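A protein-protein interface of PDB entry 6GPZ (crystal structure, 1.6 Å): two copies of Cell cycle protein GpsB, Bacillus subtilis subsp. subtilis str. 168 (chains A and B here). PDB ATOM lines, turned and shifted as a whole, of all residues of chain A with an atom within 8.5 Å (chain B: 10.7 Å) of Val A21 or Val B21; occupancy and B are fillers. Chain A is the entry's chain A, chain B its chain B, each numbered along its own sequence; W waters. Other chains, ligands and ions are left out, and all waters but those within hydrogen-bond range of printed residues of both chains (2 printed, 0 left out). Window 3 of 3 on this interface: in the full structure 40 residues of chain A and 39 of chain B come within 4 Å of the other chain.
Lys A18 touches Tyr B24 (O to CA, 3.5 Å).
Val B21 touches Val A21.
Arg A22 touches Gly B20.
Gly A23 touches Thr B19 (O to CA, 3.1 Å).
Gly A23 touches Gly B23 (CA to C, 3.5 Å).
Gly A23 touches Tyr B24.
Gly A23 touches Gln B26 (CA to OE1, 3.8 Å).
Tyr A24 touches Gln B26 (CZ to CG, 3.5 Å).
CD of Lys A25 touches O of Thr B19 (3.9 Å).
NZ of Lys A25 touches CA of Gly B20 (3.96 Å).
The backbone carbonyl oxygen (O) of Lys B18 lies within hydrogen-bond range of the backbone NH (N) of Lys A25 (2.9 Å).
The backbone NH (N) of Gly B20 lies within hydrogen-bond range of the backbone carbonyl oxygen (O) of Gly A23, at 2.9 Å.
The side-chain hydroxyl (OG1) of Thr A19 lies within hydrogen-bond range of the guanidinium group (NH1) of Arg B22.
The backbone carbonyl oxygen of Gly A20 lies close to the guanidinium group of Arg B22.
The backbone carbonyl oxygen (O) of Val A21 is in hydrogen-bond range of the backbone NH (N) of Arg B22.
OE1 of Gln A26 lies close to O of Arg B22.
The backbone carbonyl oxygen (O) of Gly B23 lies within hydrogen-bond range of the backbone NH (N) of Gly A20 (3.0 Å).
O of Tyr B24 lies within hydrogen-bond range of N of Tyr A24.
The backbone carbonyl oxygen (O) of Lys A18 lies within hydrogen-bond range of the backbone NH (N) of Lys B25, at 2.8 Å.
Gly A20 touches Arg B22, and with the chains exchanged Arg A22 touches Gly B20.
Gly A23 touches Tyr B24, and with the chains exchanged Tyr A24 touches Gly B23.
Gly A23 touches Gln B26, but with the chains exchanged Gln A26 does not touch Gly B23 (4.3 Å).
Tyr A24 touches Gln B26, and with the chains exchanged Gln A26 touches Tyr B24.
Water W1 lies within hydrogen-bond range of OG1 of Thr B19 and NH2 of Arg A22.
Water W2 lies within hydrogen-bond range of O of Thr B19 (2.7 Å) and NZ of Lys A25 (2.9 Å).
Hydrophobic or aromatic side chains of chain A within 4 Å of the printed part of chain B: Val A21 and Tyr A24.
Among the printed residues, no Asp or Glu carboxylate lies within 4 Å of a Lys or Arg side-chain nitrogen of the other chain.
Gly A20 touches just these residues of chain B: Arg B22 and Gly B23.
Val A21 touches just these residues of chain B: Val B21 (3.5 Å) and Arg B22 (2.9 Å).
Printed residues of chain A within 4 Å of Gly B20: Arg A22 (3.4 Å), Gly A23 (2.9 Å) and Lys A25 (3.96 Å).
Of chain A, only Val A21 (3.5 Å) comes within 4 Å of Val B21.
Printed residues of chain A within 4 Å of Arg B22: Thr A19, Gly A20, Val A21 and Gln A26.
Printed residues of chain A within 4 Å of Gln B26: Gly A23 (3.8 Å) and Tyr A24 (3.5 Å).
The nearest residue of chain B that does not touch Val A21 is Gly B20 (4.3 Å).
The nearest residue of chain A that does not touch Val B21 is Arg A22 (4.5 Å).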
ATOM      1  N   LYS A  18      21.745 -12.052  -6.916  1.00  0.00           N
ATOM      2  CA  LYS A  18      21.556 -11.714  -5.502  1.00  0.00           C
ATOM      3  C   LYS A  18      21.658 -12.978  -4.654  1.00  0.00           C
ATOM      4  O   LYS A  18      21.362 -14.073  -5.131  1.00  0.00           O
ATOM      5  CB  LYS A  18      20.183 -11.084  -5.292  1.00  0.00           C
ATOM      6  CG  LYS A  18      20.116  -9.643  -5.762  1.00  0.00           C
ATOM      7  N   THR A  19      22.055 -12.812  -3.378  1.00  0.00           N
ATOM      8  CA  THR A  19      22.061 -13.958  -2.471  1.00  0.00           C
ATOM      9  C   THR A  19      20.889 -13.824  -1.525  1.00  0.00           C
ATOM     10  O   THR A  19      20.352 -12.743  -1.353  1.00  0.00           O
ATOM     11  CB  THR A  19      23.334 -14.055  -1.655  1.00  0.00           C
ATOM     12  OG1 THR A  19      23.497 -12.880  -0.860  1.00  0.00           O
ATOM     13  CG2 THR A  19      24.549 -14.336  -2.591  1.00  0.00           C
ATOM     14  N   GLY A  20      20.468 -14.959  -0.956  1.00  0.00           N
ATOM     15  CA  GLY A  20      19.450 -14.944   0.085  1.00  0.00           C
ATOM     16  C   GLY A  20      20.032 -15.504   1.370  1.00  0.00           C
ATOM     17  O   GLY A  20      21.186 -15.934   1.415  1.00  0.00           O
ATOM     18  N   VAL A  21      19.239 -15.458   2.426  1.00  0.00           N
ATOM     19  CA  VAL A  21      19.684 -16.175   3.627  1.00  0.00           C
ATOM     20  C   VAL A  21      20.018 -17.602   3.253  1.00  0.00           C
ATOM     21  O   VAL A  21      20.973 -18.207   3.766  1.00  0.00           O
ATOM     22  CB  VAL A  21      18.588 -16.142   4.698  1.00  0.00           C
ATOM     23  CG1 VAL A  21      18.903 -17.053   5.888  1.00  0.00           C
ATOM     24  CG2 VAL A  21      18.329 -14.691   5.218  1.00  0.00           C
ATOM     25  N   ARG A  22      19.146 -18.209   2.427  1.00  0.00           N
ATOM     26  CA  ARG A  22      19.455 -19.453   1.714  1.00  0.00           C
ATOM     27  C   ARG A  22      19.260 -19.249   0.224  1.00  0.00           C
ATOM     28  O   ARG A  22      18.469 -18.385  -0.213  1.00  0.00           O
ATOM     29  CB  ARG A  22      18.556 -20.623   2.143  1.00  0.00           C
ATOM     30  CG  ARG A  22      18.752 -20.992   3.563  1.00  0.00           C
ATOM     31  CD  ARG A  22      17.616 -21.940   4.038  1.00  0.00           C
ATOM     32  NE  ARG A  22      17.972 -23.324   3.565  1.00  0.00           N
ATOM     33  CZ  ARG A  22      17.023 -24.234   3.311  1.00  0.00           C
ATOM     34  NH1 ARG A  22      15.751 -23.868   3.335  1.00  0.00           N
ATOM     35  NH2 ARG A  22      17.360 -25.507   3.012  1.00  0.00           N
ATOM     36  N   GLY A  23      19.921 -20.096  -0.538  1.00  0.00           N
ATOM     37  CA  GLY A  23      19.743 -20.107  -1.991  1.00  0.00           C
ATOM     38  C   GLY A  23      20.416 -21.309  -2.575  1.00  0.00           C
ATOM     39  O   GLY A  23      20.878 -22.171  -1.854  1.00  0.00           O
ATOM     40  N   TYR A  24      20.511 -21.350  -3.918  1.00  0.00           N
ATOM     41  CA  TYR A  24      21.264 -22.443  -4.535  1.00  0.00           C
ATOM     42  C   TYR A  24      22.758 -22.343  -4.200  1.00  0.00           C
ATOM     43  O   TYR A  24      23.369 -21.253  -4.193  1.00  0.00           O
ATOM     44  CB  TYR A  24      21.123 -22.366  -6.042  1.00  0.00           C
ATOM     45  CG  TYR A  24      19.780 -22.633  -6.664  1.00  0.00           C
ATOM     46  CD1 TYR A  24      18.980 -23.679  -6.227  1.00  0.00           C
ATOM     47  CD2 TYR A  24      19.379 -21.913  -7.808  1.00  0.00           C
ATOM     48  CE1 TYR A  24      17.781 -23.992  -6.909  1.00  0.00           C
ATOM     49  CE2 TYR A  24      18.162 -22.193  -8.436  1.00  0.00           C
ATOM     50  CZ  TYR A  24      17.377 -23.223  -7.989  1.00  0.00           C
ATOM     51  OH  TYR A  24      16.170 -23.585  -8.584  1.00  0.00           O
ATOM     52  N   LYS A  25      23.374 -23.472  -3.924  1.00  0.00           N
ATOM     53  CA  LYS A  25      24.756 -23.460  -3.500  1.00  0.00           C
ATOM     54  C   LYS A  25      25.610 -22.823  -4.605  1.00  0.00           C
ATOM     55  O   LYS A  25      25.537 -23.243  -5.768  1.00  0.00           O
ATOM     56  CB  LYS A  25      25.188 -24.893  -3.290  1.00  0.00           C
ATOM     57  CG  LYS A  25      26.404 -25.091  -2.370  1.00  0.00           C
ATOM     58  CD  LYS A  25      26.041 -24.795  -0.912  1.00  0.00           C
ATOM     59  CE  LYS A  25      27.228 -25.005   0.010  1.00  0.00           C
ATOM     60  NZ  LYS A  25      26.705 -24.912   1.482  1.00  0.00           N
ATOM     61  N   GLN A  26      26.400 -21.820  -4.249  1.00  0.00           N
ATOM     62  CA  GLN A  26      27.089 -21.064  -5.301  1.00  0.00           C
ATOM     63  C   GLN A  26      28.079 -21.917  -6.093  1.00  0.00           C
ATOM     64  O   GLN A  26      28.237 -21.743  -7.314  1.00  0.00           O
ATOM     65  CB  GLN A  26      27.847 -19.931  -4.675  1.00  0.00           C
ATOM     66  CG  GLN A  26      26.853 -18.833  -4.135  1.00  0.00           C
ATOM     67  CD  GLN A  26      27.550 -17.554  -3.691  1.00  0.00           C
ATOM     68  OE1 GLN A  26      27.087 -16.815  -2.720  1.00  0.00           O
ATOM     69  NE2 GLN A  26      28.642 -17.240  -4.305  1.00  0.00           N
ATOM     70  N   LYS B  18      21.592 -28.263  -5.096  1.00  0.00           N
ATOM     71  CA  LYS B  18      21.315 -28.236  -3.676  1.00  0.00           C
ATOM     72  C   LYS B  18      21.393 -26.804  -3.182  1.00  0.00           C
ATOM     73  O   LYS B  18      21.856 -25.892  -3.883  1.00  0.00           O
ATOM     74  CB  LYS B  18      22.275 -29.102  -2.911  1.00  0.00           C
ATOM     75  CG  LYS B  18      23.657 -28.601  -2.823  1.00  0.00           C
ATOM     76  CD  LYS B  18      24.526 -29.577  -2.041  1.00  0.00           C
ATOM     77  CE  LYS B  18      25.956 -29.193  -2.079  1.00  0.00           C
ATOM     78  NZ  LYS B  18      26.631 -29.804  -3.312  1.00  0.00           N
ATOM     79  N   THR B  19      20.924 -26.626  -1.965  1.00  0.00           N
ATOM     80  CA  THR B  19      20.886 -25.283  -1.368  1.00  0.00           C
ATOM     81  C   THR B  19      21.933 -25.156  -0.279  1.00  0.00           C
ATOM     82  O   THR B  19      22.589 -26.133   0.146  1.00  0.00           O
ATOM     83  CB  THR B  19      19.476 -24.959  -0.833  1.00  0.00           C
ATOM     84  OG1 THR B  19      19.021 -26.062  -0.057  1.00  0.00           O
ATOM     85  CG2 THR B  19      18.467 -24.759  -2.017  1.00  0.00           C
ATOM     86  N   GLY B  20      22.064 -23.898   0.190  1.00  0.00           N
ATOM     87  CA  GLY B  20      22.965 -23.636   1.308  1.00  0.00           C
ATOM     88  C   GLY B  20      22.823 -22.213   1.775  1.00  0.00           C
ATOM     89  O   GLY B  20      22.126 -21.413   1.146  1.00  0.00           O
ATOM     90  N   VAL B  21      23.531 -21.910   2.865  1.00  0.00           N
ATOM     91  CA  VAL B  21      23.497 -20.540   3.427  1.00  0.00           C
ATOM     92  C   VAL B  21      24.094 -19.560   2.406  1.00  0.00           C
ATOM     93  O   VAL B  21      25.122 -19.817   1.758  1.00  0.00           O
ATOM     94  CB  VAL B  21      24.240 -20.514   4.768  1.00  0.00           C
ATOM     95  CG1 VAL B  21      25.761 -20.704   4.638  1.00  0.00           C
ATOM     96  CG2 VAL B  21      24.018 -19.136   5.485  1.00  0.00           C
ATOM     97  N   ARG B  22      23.460 -18.393   2.298  1.00  0.00           N
ATOM     98  CA  ARG B  22      23.915 -17.324   1.372  1.00  0.00           C
ATOM     99  C   ARG B  22      24.065 -17.839  -0.065  1.00  0.00           C
ATOM    100  O   ARG B  22      24.881 -17.335  -0.872  1.00  0.00           O
ATOM    101  CB  ARG B  22      25.176 -16.665   1.915  1.00  0.00           C
ATOM    102  CG  ARG B  22      24.850 -15.770   3.155  1.00  0.00           C
ATOM    103  CD  ARG B  22      24.145 -14.435   2.714  1.00  0.00           C
ATOM    104  NE  ARG B  22      23.149 -13.950   3.634  1.00  0.00           N
ATOM    105  CZ  ARG B  22      22.146 -13.164   3.281  1.00  0.00           C
ATOM    106  NH1 ARG B  22      22.049 -12.734   1.992  1.00  0.00           N
ATOM    107  NH2 ARG B  22      21.284 -12.788   4.195  1.00  0.00           N
ATOM    108  N   GLY B  23      23.291 -18.849  -0.445  1.00  0.00           N
ATOM    109  CA  GLY B  23      23.259 -19.255  -1.824  1.00  0.00           C
ATOM    110  C   GLY B  23      22.610 -18.180  -2.717  1.00  0.00           C
ATOM    111  O   GLY B  23      22.015 -17.182  -2.300  1.00  0.00           O
ATOM    112  N   TYR B  24      22.773 -18.404  -4.025  1.00  0.00           N
ATOM    113  CA  TYR B  24      22.181 -17.486  -4.992  1.00  0.00           C
ATOM    114  C   TYR B  24      20.665 -17.610  -4.962  1.00  0.00           C
ATOM    115  O   TYR B  24      20.128 -18.713  -4.887  1.00  0.00           O
ATOM    116  CB  TYR B  24      22.670 -17.858  -6.374  1.00  0.00           C
ATOM    117  CG  TYR B  24      24.124 -17.720  -6.686  1.00  0.00           C
ATOM    118  CD1 TYR B  24      24.851 -16.574  -6.356  1.00  0.00           C
ATOM    119  CD2 TYR B  24      24.744 -18.715  -7.462  1.00  0.00           C
ATOM    120  CE1 TYR B  24      26.166 -16.443  -6.741  1.00  0.00           C
ATOM    121  CE2 TYR B  24      26.051 -18.578  -7.864  1.00  0.00           C
ATOM    122  CZ  TYR B  24      26.768 -17.434  -7.537  1.00  0.00           C
ATOM    123  OH  TYR B  24      28.069 -17.241  -7.935  1.00  0.00           O
ATOM    124  N   LYS B  25      19.971 -16.465  -5.020  1.00  0.00           N
ATOM    125  CA  LYS B  25      18.518 -16.428  -5.038  1.00  0.00           C
ATOM    126  C   LYS B  25      17.997 -17.298  -6.164  1.00  0.00           C
ATOM    127  O   LYS B  25      18.416 -17.144  -7.301  1.00  0.00           O
ATOM    128  CB  LYS B  25      18.064 -14.951  -5.187  1.00  0.00           C
ATOM    129  CG  LYS B  25      16.589 -14.661  -4.931  1.00  0.00           C
ATOM    130  CD  LYS B  25      16.216 -13.134  -4.729  1.00  0.00           C
ATOM    131  N   GLN B  26      17.076 -18.192  -5.836  1.00  0.00           N
ATOM    132  CA  GLN B  26      16.684 -19.201  -6.820  1.00  0.00           C
ATOM    133  C   GLN B  26      16.059 -18.578  -8.037  1.00  0.00           C
ATOM    134  O   GLN B  26      16.358 -18.977  -9.155  1.00  0.00           O
ATOM    135  CB  GLN B  26      15.706 -20.200  -6.192  1.00  0.00           C
ATOM    136  CG  GLN B  26      16.406 -21.200  -5.317  1.00  0.00           C
ATOM    137  CD  GLN B  26      16.343 -20.861  -3.897  1.00  0.00           C
ATOM    138  OE1 GLN B  26      16.321 -19.672  -3.523  1.00  0.00           O
ATOM    139  NE2 GLN B  26      16.256 -21.916  -3.050  1.00  0.00           N
HETATM  140  O   HOH W   1      20.015 -26.405   2.380  1.00  0.00           O
HETATM  141  O   HOH W   2      24.551 -26.770   1.911  1.00  0.00           O
